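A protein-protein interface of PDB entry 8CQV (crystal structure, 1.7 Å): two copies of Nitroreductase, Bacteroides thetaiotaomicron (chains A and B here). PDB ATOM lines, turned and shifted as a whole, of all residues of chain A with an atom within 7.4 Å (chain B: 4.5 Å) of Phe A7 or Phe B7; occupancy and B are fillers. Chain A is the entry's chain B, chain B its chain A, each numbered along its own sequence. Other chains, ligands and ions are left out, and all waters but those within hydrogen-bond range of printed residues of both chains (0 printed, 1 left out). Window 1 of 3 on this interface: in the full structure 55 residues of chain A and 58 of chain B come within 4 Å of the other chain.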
ATOM      1  N   GLU A   4      18.605 -19.529 -25.228  1.00  0.00           N
ATOM      2  CA  GLU A   4      19.466 -19.891 -24.071  1.00  0.00           C
ATOM      3  C   GLU A   4      20.888 -20.175 -24.547  1.00  0.00           C
ATOM      4  O   GLU A   4      21.082 -20.792 -25.587  1.00  0.00           O
ATOM      5  CB  GLU A   4      18.961 -21.212 -23.489  1.00  0.00           C
ATOM      6  CG  GLU A   4      18.231 -21.128 -22.180  1.00  0.00           C
ATOM      7  CD  GLU A   4      18.068 -22.495 -21.520  1.00  0.00           C
ATOM      8  OE1 GLU A   4      17.299 -23.330 -21.979  1.00  0.00           O
ATOM      9  OE2 GLU A   4      18.645 -22.701 -20.567  1.00  0.00           O
ATOM     10  N   ARG A   5      21.897 -19.807 -23.756  1.00  0.00           N
ATOM     11  CA  ARG A   5      23.282 -20.129 -24.104  1.00  0.00           C
ATOM     12  C   ARG A   5      23.548 -21.627 -23.809  1.00  0.00           C
ATOM     13  O   ARG A   5      22.667 -22.293 -23.292  1.00  0.00           O
ATOM     14  CB  ARG A   5      24.177 -19.201 -23.295  1.00  0.00           C
ATOM     15  CG  ARG A   5      23.956 -17.723 -23.561  1.00  0.00           C
ATOM     16  CD  ARG A   5      24.694 -17.026 -22.437  1.00  0.00           C
ATOM     17  NE  ARG A   5      24.716 -15.587 -22.560  1.00  0.00           N
ATOM     18  CZ  ARG A   5      23.653 -14.791 -22.551  1.00  0.00           C
ATOM     19  NH1 ARG A   5      22.490 -15.208 -22.084  1.00  0.00           N
ATOM     20  NH2 ARG A   5      23.772 -13.542 -22.970  1.00  0.00           N
ATOM     21  N   THR A   6      24.753 -22.153 -24.037  1.00  0.00           N
ATOM     22  CA  THR A   6      25.134 -23.439 -23.430  1.00  0.00           C
ATOM     23  C   THR A   6      25.262 -23.284 -21.929  1.00  0.00           C
ATOM     24  O   THR A   6      25.342 -22.173 -21.432  1.00  0.00           O
ATOM     25  CB  THR A   6      26.409 -24.043 -24.040  1.00  0.00           C
ATOM     26  OG1 THR A   6      27.469 -23.159 -23.680  1.00  0.00           O
ATOM     27  CG2 THR A   6      26.324 -24.205 -25.546  1.00  0.00           C
ATOM     28  N   PHE A   7      25.219 -24.396 -21.204  1.00  0.00           N
ATOM     29  CA  PHE A   7      25.370 -24.411 -19.762  1.00  0.00           C
ATOM     30  C   PHE A   7      26.604 -23.588 -19.359  1.00  0.00           C
ATOM     31  O   PHE A   7      26.518 -22.746 -18.490  1.00  0.00           O
ATOM     32  CB  PHE A   7      25.414 -25.845 -19.207  1.00  0.00           C
ATOM     33  CG  PHE A   7      25.561 -25.859 -17.708  1.00  0.00           C
ATOM     34  CD1 PHE A   7      26.816 -25.729 -17.111  1.00  0.00           C
ATOM     35  CD2 PHE A   7      24.479 -25.997 -16.870  1.00  0.00           C
ATOM     36  CE1 PHE A   7      26.952 -25.710 -15.723  1.00  0.00           C
ATOM     37  CE2 PHE A   7      24.640 -25.965 -15.478  1.00  0.00           C
ATOM     38  CZ  PHE A   7      25.884 -25.799 -14.926  1.00  0.00           C
ATOM     39  N   SER A   8      27.746 -23.863 -19.968  1.00  0.00           N
ATOM     40  CA  SER A   8      29.009 -23.251 -19.516  1.00  0.00           C
ATOM     41  C   SER A   8      29.019 -21.765 -19.839  1.00  0.00           C
ATOM     42  O   SER A   8      29.487 -20.985 -19.040  1.00  0.00           O
ATOM     43  CB  SER A   8      30.234 -24.001 -20.043  1.00  0.00           C
ATOM     44  OG  SER A   8      30.377 -23.857 -21.404  1.00  0.00           O
ATOM     45  N   GLU A   9      28.391 -21.372 -20.960  1.00  0.00           N
ATOM     46  CA  GLU A   9      28.348 -19.987 -21.369  1.00  0.00           C
ATOM     47  C   GLU A   9      27.432 -19.224 -20.420  1.00  0.00           C
ATOM     48  O   GLU A   9      27.755 -18.122 -19.998  1.00  0.00           O
ATOM     49  CB  GLU A   9      27.914 -19.860 -22.822  1.00  0.00           C
ATOM     50  CG  GLU A   9      29.046 -20.125 -23.808  1.00  0.00           C
ATOM     51  CD  GLU A   9      29.997 -18.932 -23.842  1.00  0.00           C
ATOM     52  OE1 GLU A   9      29.580 -17.848 -24.365  1.00  0.00           O
ATOM     53  OE2 GLU A   9      31.100 -19.038 -23.246  1.00  0.00           O
ATOM     54  N   ALA A  10      26.268 -19.828 -20.110  1.00  0.00           N
ATOM     55  CA  ALA A  10      25.337 -19.224 -19.172  1.00  0.00           C
ATOM     56  C   ALA A  10      25.999 -19.039 -17.785  1.00  0.00           C
ATOM     57  O   ALA A  10      25.875 -18.029 -17.118  1.00  0.00           O
ATOM     58  CB  ALA A  10      24.072 -20.095 -19.153  1.00  0.00           C
ATOM     59  N   LEU A  11      26.722 -20.061 -17.324  1.00  0.00           N
ATOM     60  CA  LEU A  11      27.453 -19.988 -16.070  1.00  0.00           C
ATOM     61  C   LEU A  11      28.490 -18.868 -16.088  1.00  0.00           C
ATOM     62  O   LEU A  11      28.579 -18.087 -15.137  1.00  0.00           O
ATOM     63  CB  LEU A  11      28.080 -21.361 -15.788  1.00  0.00           C
ATOM     64  CG  LEU A  11      28.768 -21.555 -14.453  1.00  0.00           C
ATOM     65  CD1 LEU A  11      27.751 -21.542 -13.329  1.00  0.00           C
ATOM     66  CD2 LEU A  11      29.613 -22.819 -14.415  1.00  0.00           C
ATOM     67  N   LYS A  12      29.294 -18.783 -17.134  1.00  0.00           N
ATOM     68  CA  LYS A  12      30.296 -17.720 -17.195  1.00  0.00           C
ATOM     69  C   LYS A  12      29.664 -16.319 -17.303  1.00  0.00           C
ATOM     70  O   LYS A  12      30.232 -15.368 -16.789  1.00  0.00           O
ATOM     71  CB  LYS A  12      31.232 -18.019 -18.355  1.00  0.00           C
ATOM     72  CG  LYS A  12      32.339 -17.014 -18.611  1.00  0.00           C
ATOM     73  CD  LYS A  12      33.096 -17.274 -19.976  1.00  0.00           C
ATOM     74  CE  LYS A  12      33.140 -18.742 -20.385  1.00  0.00           C
ATOM     75  NZ  LYS A  12      34.082 -18.985 -21.508  1.00  0.00           N
ATOM     76  N   ASN A  13      28.485 -16.196 -17.940  1.00  0.00           N
ATOM     77  CA  ASN A  13      27.759 -14.936 -18.106  1.00  0.00           C
ATOM     78  C   ASN A  13      27.272 -14.369 -16.765  1.00  0.00           C
ATOM     79  O   ASN A  13      27.091 -13.142 -16.659  1.00  0.00           O
ATOM     80  CB  ASN A  13      26.526 -15.163 -18.997  1.00  0.00           C
ATOM     81  CG  ASN A  13      25.637 -13.965 -19.271  1.00  0.00           C
ATOM     82  OD1 ASN A  13      24.454 -13.941 -18.889  1.00  0.00           O
ATOM     83  ND2 ASN A  13      26.173 -12.996 -19.990  1.00  0.00           N
ATOM     84  N   LEU A  37      11.480 -25.069 -13.070  1.00  0.00           N
ATOM     85  CA  LEU A  37      12.508 -25.934 -13.587  1.00  0.00           C
ATOM     86  C   LEU A  37      13.546 -26.222 -12.478  1.00  0.00           C
ATOM     87  O   LEU A  37      13.871 -27.369 -12.278  1.00  0.00           O
ATOM     88  CB  LEU A  37      13.126 -25.335 -14.861  1.00  0.00           C
ATOM     89  CG  LEU A  37      13.914 -26.378 -15.648  1.00  0.00           C
ATOM     90  CD1 LEU A  37      13.458 -26.531 -17.072  1.00  0.00           C
ATOM     91  CD2 LEU A  37      15.386 -26.086 -15.547  1.00  0.00           C
ATOM     92  N   VAL A  42      16.730 -29.581  -9.448  1.00  0.00           N
ATOM     93  CA  VAL A  42      17.908 -29.410  -8.614  1.00  0.00           C
ATOM     94  C   VAL A  42      17.861 -30.470  -7.542  1.00  0.00           C
ATOM     95  O   VAL A  42      16.845 -30.646  -6.892  1.00  0.00           O
ATOM     96  CB  VAL A  42      18.066 -27.990  -8.064  1.00  0.00           C
ATOM     97  CG1 VAL A  42      19.140 -27.907  -6.988  1.00  0.00           C
ATOM     98  CG2 VAL A  42      18.349 -27.020  -9.207  1.00  0.00           C
ATOM     99  N   MET A 132      22.346 -24.642  -4.392  1.00  0.00           N
ATOM    100  CA  MET A 132      22.257 -25.181  -5.748  1.00  0.00           C
ATOM    101  C   MET A 132      21.061 -24.516  -6.504  1.00  0.00           C
ATOM    102  O   MET A 132      21.217 -24.137  -7.647  1.00  0.00           O
ATOM    103  CB  MET A 132      22.143 -26.698  -5.772  1.00  0.00           C
ATOM    104  CG  MET A 132      23.388 -27.458  -5.295  1.00  0.00           C
ATOM    105  SD  MET A 132      23.143 -29.168  -5.370  1.00  0.00           S
ATOM    106  CE  MET A 132      24.695 -29.847  -4.759  1.00  0.00           C
ATOM    107  N   LEU A 135      22.066 -20.873  -7.361  1.00  0.00           N
ATOM    108  CA  LEU A 135      22.884 -20.764  -8.540  1.00  0.00           C
ATOM    109  C   LEU A 135      22.044 -21.007  -9.803  1.00  0.00           C
ATOM    110  O   LEU A 135      22.158 -20.209 -10.706  1.00  0.00           O
ATOM    111  CB  LEU A 135      24.071 -21.745  -8.489  1.00  0.00           C
ATOM    112  CG  LEU A 135      24.950 -21.709  -9.762  1.00  0.00           C
ATOM    113  CD1 LEU A 135      25.740 -20.418  -9.800  1.00  0.00           C
ATOM    114  CD2 LEU A 135      25.905 -22.891  -9.834  1.00  0.00           C
ATOM    115  N   ALA A 136      21.203 -22.013  -9.840  1.00  0.00           N
ATOM    116  CA  ALA A 136      20.424 -22.349 -11.050  1.00  0.00           C
ATOM    117  C   ALA A 136      19.510 -21.185 -11.428  1.00  0.00           C
ATOM    118  O   ALA A 136      19.447 -20.764 -12.571  1.00  0.00           O
ATOM    119  CB  ALA A 136      19.597 -23.578 -10.721  1.00  0.00           C
ATOM    120  N   VAL A 137      18.786 -20.648 -10.452  1.00  0.00           N
ATOM    121  CA  VAL A 137      17.900 -19.503 -10.700  1.00  0.00           C
ATOM    122  C   VAL A 137      18.703 -18.298 -11.168  1.00  0.00           C
ATOM    123  O   VAL A 137      18.293 -17.610 -12.103  1.00  0.00           O
ATOM    124  CB  VAL A 137      17.006 -19.221  -9.503  1.00  0.00           C
ATOM    125  CG1 VAL A 137      16.171 -17.930  -9.654  1.00  0.00           C
ATOM    126  CG2 VAL A 137      16.083 -20.383  -9.241  1.00  0.00           C
ATOM    127  N   TRP A 138      19.792 -17.965 -10.440  1.00  0.00           N
ATOM    128  CA  TRP A 138      20.615 -16.812 -10.730  1.00  0.00           C
ATOM    129  C   TRP A 138      21.073 -16.836 -12.193  1.00  0.00           C
ATOM    130  O   TRP A 138      20.918 -15.861 -12.937  1.00  0.00           O
ATOM    131  CB  TRP A 138      21.808 -16.745  -9.768  1.00  0.00           C
ATOM    132  CG  TRP A 138      22.547 -15.476  -9.625  1.00  0.00           C
ATOM    133  CD1 TRP A 138      22.371 -14.303 -10.307  1.00  0.00           C
ATOM    134  CD2 TRP A 138      23.496 -15.181  -8.587  1.00  0.00           C
ATOM    135  NE1 TRP A 138      23.240 -13.342  -9.845  1.00  0.00           N
ATOM    136  CE2 TRP A 138      23.927 -13.849  -8.787  1.00  0.00           C
ATOM    137  CE3 TRP A 138      24.084 -15.925  -7.553  1.00  0.00           C
ATOM    138  CZ2 TRP A 138      24.884 -13.245  -7.983  1.00  0.00           C
ATOM    139  CZ3 TRP A 138      25.033 -15.317  -6.739  1.00  0.00           C
ATOM    140  CH2 TRP A 138      25.450 -14.004  -6.978  1.00  0.00           C
ATOM    141  N   VAL A 139      21.603 -18.011 -12.624  1.00  0.00           N
ATOM    142  CA  VAL A 139      22.082 -18.180 -13.983  1.00  0.00           C
ATOM    143  C   VAL A 139      20.945 -18.040 -14.964  1.00  0.00           C
ATOM    144  O   VAL A 139      21.065 -17.353 -15.950  1.00  0.00           O
ATOM    145  CB  VAL A 139      22.836 -19.538 -14.147  1.00  0.00           C
ATOM    146  CG1 VAL A 139      23.243 -19.745 -15.578  1.00  0.00           C
ATOM    147  CG2 VAL A 139      24.031 -19.562 -13.216  1.00  0.00           C
ATOM    148  N   MET A 140      19.808 -18.737 -14.720  1.00  0.00           N
ATOM    149  CA  MET A 140      18.745 -18.688 -15.732  1.00  0.00           C
ATOM    150  C   MET A 140      18.103 -17.311 -15.823  1.00  0.00           C
ATOM    151  O   MET A 140      17.760 -16.887 -16.899  1.00  0.00           O
ATOM    152  CB  MET A 140      17.671 -19.739 -15.418  1.00  0.00           C
ATOM    153  CG  MET A 140      18.199 -21.170 -15.728  1.00  0.00           C
ATOM    154  SD  MET A 140      16.849 -22.403 -15.499  1.00  0.00           S
ATOM    155  CE  MET A 140      16.731 -22.595 -13.716  1.00  0.00           C
ATOM    156  N   ASP A 143      20.383 -15.433 -17.965  1.00  0.00           N
ATOM    157  CA  ASP A 143      20.366 -15.965 -19.315  1.00  0.00           C
ATOM    158  C   ASP A 143      19.239 -15.329 -20.145  1.00  0.00           C
ATOM    159  O   ASP A 143      19.411 -15.154 -21.353  1.00  0.00           O
ATOM    160  CB  ASP A 143      20.232 -17.485 -19.278  1.00  0.00           C
ATOM    161  CG  ASP A 143      20.805 -18.161 -20.524  1.00  0.00           C
ATOM    162  OD1 ASP A 143      21.601 -17.517 -21.302  1.00  0.00           O
ATOM    163  OD2 ASP A 143      20.543 -19.336 -20.671  1.00  0.00           O
ATOM    164  N   GLU B   4      27.619 -29.232 -26.016  1.00  0.00           N
ATOM    165  CA  GLU B   4      26.882 -28.835 -24.820  1.00  0.00           C
ATOM    166  C   GLU B   4      25.393 -28.644 -25.100  1.00  0.00           C
ATOM    167  O   GLU B   4      25.026 -28.176 -26.176  1.00  0.00           O
ATOM    168  CB  GLU B   4      27.349 -27.490 -24.294  1.00  0.00           C
ATOM    169  CG  GLU B   4      28.478 -27.617 -23.299  1.00  0.00           C
ATOM    170  CD  GLU B   4      28.777 -26.330 -22.567  1.00  0.00           C
ATOM    171  OE1 GLU B   4      28.303 -26.220 -21.451  1.00  0.00           O
ATOM    172  OE2 GLU B   4      29.517 -25.486 -23.132  1.00  0.00           O
ATOM    173  N   ARG B   5      24.580 -28.956 -24.102  1.00  0.00           N
ATOM    174  CA  ARG B   5      23.193 -28.549 -24.055  1.00  0.00           C
ATOM    175  C   ARG B   5      23.084 -27.108 -23.544  1.00  0.00           C
ATOM    176  O   ARG B   5      24.032 -26.556 -22.948  1.00  0.00           O
ATOM    177  CB  ARG B   5      22.507 -29.502 -23.073  1.00  0.00           C
ATOM    178  CG  ARG B   5      22.405 -30.927 -23.594  1.00  0.00           C
ATOM    179  CD  ARG B   5      21.819 -31.729 -22.482  1.00  0.00           C
ATOM    180  NE  ARG B   5      21.564 -33.051 -22.982  1.00  0.00           N
ATOM    181  CZ  ARG B   5      22.430 -34.044 -23.016  1.00  0.00           C
ATOM    182  NH1 ARG B   5      23.690 -33.864 -22.656  1.00  0.00           N
ATOM    183  NH2 ARG B   5      22.005 -35.222 -23.453  1.00  0.00           N
ATOM    184  N   THR B   6      21.867 -26.543 -23.651  1.00  0.00           N
ATOM    185  CA  THR B   6      21.569 -25.265 -23.004  1.00  0.00           C
ATOM    186  C   THR B   6      21.586 -25.472 -21.496  1.00  0.00           C
ATOM    187  O   THR B   6      21.547 -26.609 -21.021  1.00  0.00           O
ATOM    188  CB  THR B   6      20.237 -24.697 -23.480  1.00  0.00           C
ATOM    189  OG1 THR B   6      19.224 -25.586 -23.024  1.00  0.00           O
ATOM    190  CG2 THR B   6      20.122 -24.545 -24.984  1.00  0.00           C
ATOM    191  N   PHE B   7      21.627 -24.385 -20.720  1.00  0.00           N
ATOM    192  CA  PHE B   7      21.734 -24.481 -19.280  1.00  0.00           C
ATOM    193  C   PHE B   7      20.560 -25.313 -18.753  1.00  0.00           C
ATOM    194  O   PHE B   7      20.767 -26.196 -17.920  1.00  0.00           O
ATOM    195  CB  PHE B   7      21.755 -23.058 -18.693  1.00  0.00           C
ATOM    196  CG  PHE B   7      21.941 -23.078 -17.186  1.00  0.00           C
ATOM    197  CD1 PHE B   7      20.873 -23.249 -16.323  1.00  0.00           C
ATOM    198  CD2 PHE B   7      23.212 -22.982 -16.643  1.00  0.00           C
ATOM    199  CE1 PHE B   7      21.095 -23.326 -14.955  1.00  0.00           C
ATOM    200  CE2 PHE B   7      23.431 -23.020 -15.271  1.00  0.00           C
ATOM    201  CZ  PHE B   7      22.358 -23.189 -14.426  1.00  0.00           C
ATOM    202  N   SER B   8      19.331 -24.964 -19.155  1.00  0.00           N
ATOM    203  CA  SER B   8      18.131 -25.613 -18.616  1.00  0.00           C
ATOM    204  C   SER B   8      18.102 -27.107 -19.003  1.00  0.00           C
ATOM    205  O   SER B   8      17.705 -27.938 -18.187  1.00  0.00           O
ATOM    206  CB  SER B   8      16.810 -24.924 -19.030  1.00  0.00           C
ATOM    207  OG  SER B   8      16.598 -25.056 -20.423  1.00  0.00           O
ATOM    208  N   GLU B   9      18.542 -27.430 -20.207  1.00  0.00           N
ATOM    209  CA  GLU B   9      18.510 -28.810 -20.693  1.00  0.00           C
ATOM    210  C   GLU B   9      19.556 -29.609 -19.927  1.00  0.00           C
ATOM    211  O   GLU B   9      19.307 -30.744 -19.552  1.00  0.00           O
ATOM    212  CB  GLU B   9      18.823 -28.856 -22.185  1.00  0.00           C
ATOM    213  CG  GLU B   9      17.729 -28.340 -23.098  1.00  0.00           C
ATOM    214  CD  GLU B   9      18.256 -28.241 -24.535  1.00  0.00           C
ATOM    215  OE1 GLU B   9      17.426 -28.033 -25.442  1.00  0.00           O
ATOM    216  OE2 GLU B   9      19.534 -28.403 -24.796  1.00  0.00           O
ATOM    217  N   ALA B  10      20.754 -29.032 -19.755  1.00  0.00           N
ATOM    218  CA  ALA B  10      21.822 -29.705 -19.000  1.00  0.00           C
ATOM    219  C   ALA B  10      21.382 -29.973 -17.547  1.00  0.00           C
ATOM    220  O   ALA B  10      21.600 -31.031 -16.955  1.00  0.00           O
ATOM    221  CB  ALA B  10      23.079 -28.832 -19.085  1.00  0.00           C
ATOM    222  N   LEU B  11      20.712 -28.989 -16.932  1.00  0.00           N
ATOM    223  CA  LEU B  11      20.242 -29.132 -15.572  1.00  0.00           C
ATOM    224  C   LEU B  11      19.199 -30.243 -15.517  1.00  0.00           C
ATOM    225  O   LEU B  11      19.249 -31.085 -14.624  1.00  0.00           O
ATOM    226  CB  LEU B  11      19.611 -27.763 -15.167  1.00  0.00           C
ATOM    227  CG  LEU B  11      19.274 -27.590 -13.708  1.00  0.00           C
ATOM    228  CD1 LEU B  11      20.534 -27.508 -12.826  1.00  0.00           C
ATOM    229  CD2 LEU B  11      18.373 -26.341 -13.521  1.00  0.00           C
ATOM    230  N   ALA B 136      27.545 -27.465 -10.558  1.00  0.00           N
ATOM    231  CA  ALA B 136      28.059 -27.070 -11.854  1.00  0.00           C
ATOM    232  C   ALA B 136      28.856 -28.236 -12.476  1.00  0.00           C
ATOM    233  O   ALA B 136      28.720 -28.579 -13.631  1.00  0.00           O
ATOM    234  CB  ALA B 136      28.954 -25.896 -11.645  1.00  0.00           C
ATOM    235  N   VAL B 139      26.577 -31.342 -13.443  1.00  0.00           N
ATOM    236  CA  VAL B 139      25.785 -31.111 -14.613  1.00  0.00           C
ATOM    237  C   VAL B 139      26.698 -31.177 -15.838  1.00  0.00           C
ATOM    238  O   VAL B 139      26.370 -31.817 -16.851  1.00  0.00           O
ATOM    239  CB  VAL B 139      25.060 -29.753 -14.526  1.00  0.00           C
ATOM    240  CG1 VAL B 139      24.468 -29.382 -15.874  1.00  0.00           C
ATOM    241  CG2 VAL B 139      23.997 -29.730 -13.443  1.00  0.00           C
ATOM    242  N   MET B 140      27.869 -30.526 -15.770  1.00  0.00           N
ATOM    243  CA  MET B 140      28.715 -30.515 -16.952  1.00  0.00           C
ATOM    244  C   MET B 140      29.303 -31.915 -17.257  1.00  0.00           C
ATOM    245  O   MET B 140      29.465 -32.290 -18.405  1.00  0.00           O
ATOM    246  CB  MET B 140      29.876 -29.524 -16.784  1.00  0.00           C
ATOM    247  CG  MET B 140      29.397 -28.125 -16.931  1.00  0.00           C
ATOM    248  SD  MET B 140      30.700 -26.861 -16.964  1.00  0.00           S
ATOM    249  CE  MET B 140      31.123 -26.704 -15.228  1.00  0.00           C
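OE1 of Glu A4 sits at hydrogen-bond distance from OG of Ser B8, at 2.4 Å.
OE2 of Glu B4 is in hydrogen-bond range of OG1 of Thr A6, at 3.1 Å.
O of Arg A5 lies within hydrogen-bond range of N of Phe B7 (3.5 Å).
OG1 of Thr B6 is in hydrogen-bond range of OE1 of Glu A4 (3.1 Å).
OE2 of Glu B4 sits at hydrogen-bond distance from OG of Ser A8, 2.5 Å away.
The backbone carbonyl oxygen (O) of Arg B5 is in hydrogen-bond range of the backbone NH (N) of Phe A7 (3.0 Å).
OE2 of Glu A4 is in hydrogen-bond range of N of Phe B7, at 3.4 Å.
OD1 of Asp A143 is in salt-bridge range of NH1 of Arg A5 (2.6 Å).
The backbone NH (N) of Glu A9 sits at hydrogen-bond distance from the side-chain hydroxyl (OG1) of Thr A6 (3.4 Å).
The backbone NH (N) of Thr B6 is in hydrogen-bond range of the side-chain carboxylate (OE2) of Glu B9 (3.2 Å).
Thr B6 touches Arg A5 (CA to O, 3.2 Å).
Thr A6 touches Phe B7 (C to N, 3.99 Å).
Thr B6 touches Phe A7.
Phe A7 touches Phe B7 (CE2 to CE2, 3.2 Å).
CB of Ala B10 touches CB of Phe A7, 3.8 Å away.
Val B139 touches Phe A7.
CD2 of Leu A37 touches CB of Ser B8 (3.9 Å).
Ala A136 touches Phe B7.
Val A139 touches Phe B7.
CD1 of Phe B7 touches CG of Met A140 (3.4 Å).
Printed residues of chain B within 4 Å of Glu A4: Thr B6 (3.1 Å), Phe B7 (3.4 Å) and Ser B8 (2.4 Å).
Printed residues of chain B within 4 Å of Thr A6: Glu B4 (3.1 Å), Arg B5 (3.3 Å) and Phe B7 (3.99 Å).
Of chain B, only Glu B4, Arg B5, Thr B6, Phe B7, Ala B10, Ala B136, Val B139 and Met B140 come within 4 Å of Phe A7.
Leu A135 touches none of the printed residues of chain B.
Printed residues of chain B within 4 Å of Val A139: Phe B7.
Of the printed residues of chain A, Arg B5 touches Thr A6 and Phe A7.
Printed residues of chain A within 4 Å of Thr B6: Glu A4, Arg A5 and Phe A7.
Of the printed residues of chain A, Phe B7 touches Glu A4 (3.4 Å), Arg A5 (3.5 Å), Thr A6 (3.99 Å), Phe A7 (3.2 Å), Ala A10 (3.8 Å), Ala A136 (3.9 Å), Val A139 (3.3 Å) and Met A140 (3.4 Å).
The nearest printed residue of chain B that does not touch Phe A7 is Leu B11 (4.8 Å).
The nearest printed residue of chain A that does not touch Phe B7 is Asp A143 (4.4 Å).
Of the 20 printed residues of chain A, 10 touch a printed residue of chain B.
Hydrophobic or aromatic side chains of chain A that line the printed part of chain B: Phe A7, Ala A10, Leu A37, Val A139 and Met A140.
Of the 11 printed residues of chain B, 10 touch a printed residue of chain A.
Hydrophobic or aromatic side chains of chain B within 4 Å of the printed part of chain A: Phe B7, Ala B10, Leu B11, Val B139 and Met B140.
Among the printed residues, no Asp or Glu carboxylate lies within 4 Å of a Lys or Arg side-chain nitrogen of the other chain.
Glu A4 touches Thr B6, and with the chains exchanged Thr A6 touches Glu B4.
Arg A5 touches Thr B6, and with the chains exchanged Thr A6 touches Arg B5.
Arg A5 touches Phe B7, and with the chains exchanged Phe A7 touches Arg B5.
Thr A6 touches Phe B7, and with the chains exchanged Phe A7 touches Thr B6.
Positions printed for both chains: 4, 5, 6, 7, 8, 9, 10, 11, 136, 139 and 140.
Of the 23 pairs that touch across the chains among the printed residues, 21 have their exchanged pair printed and touching as well.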
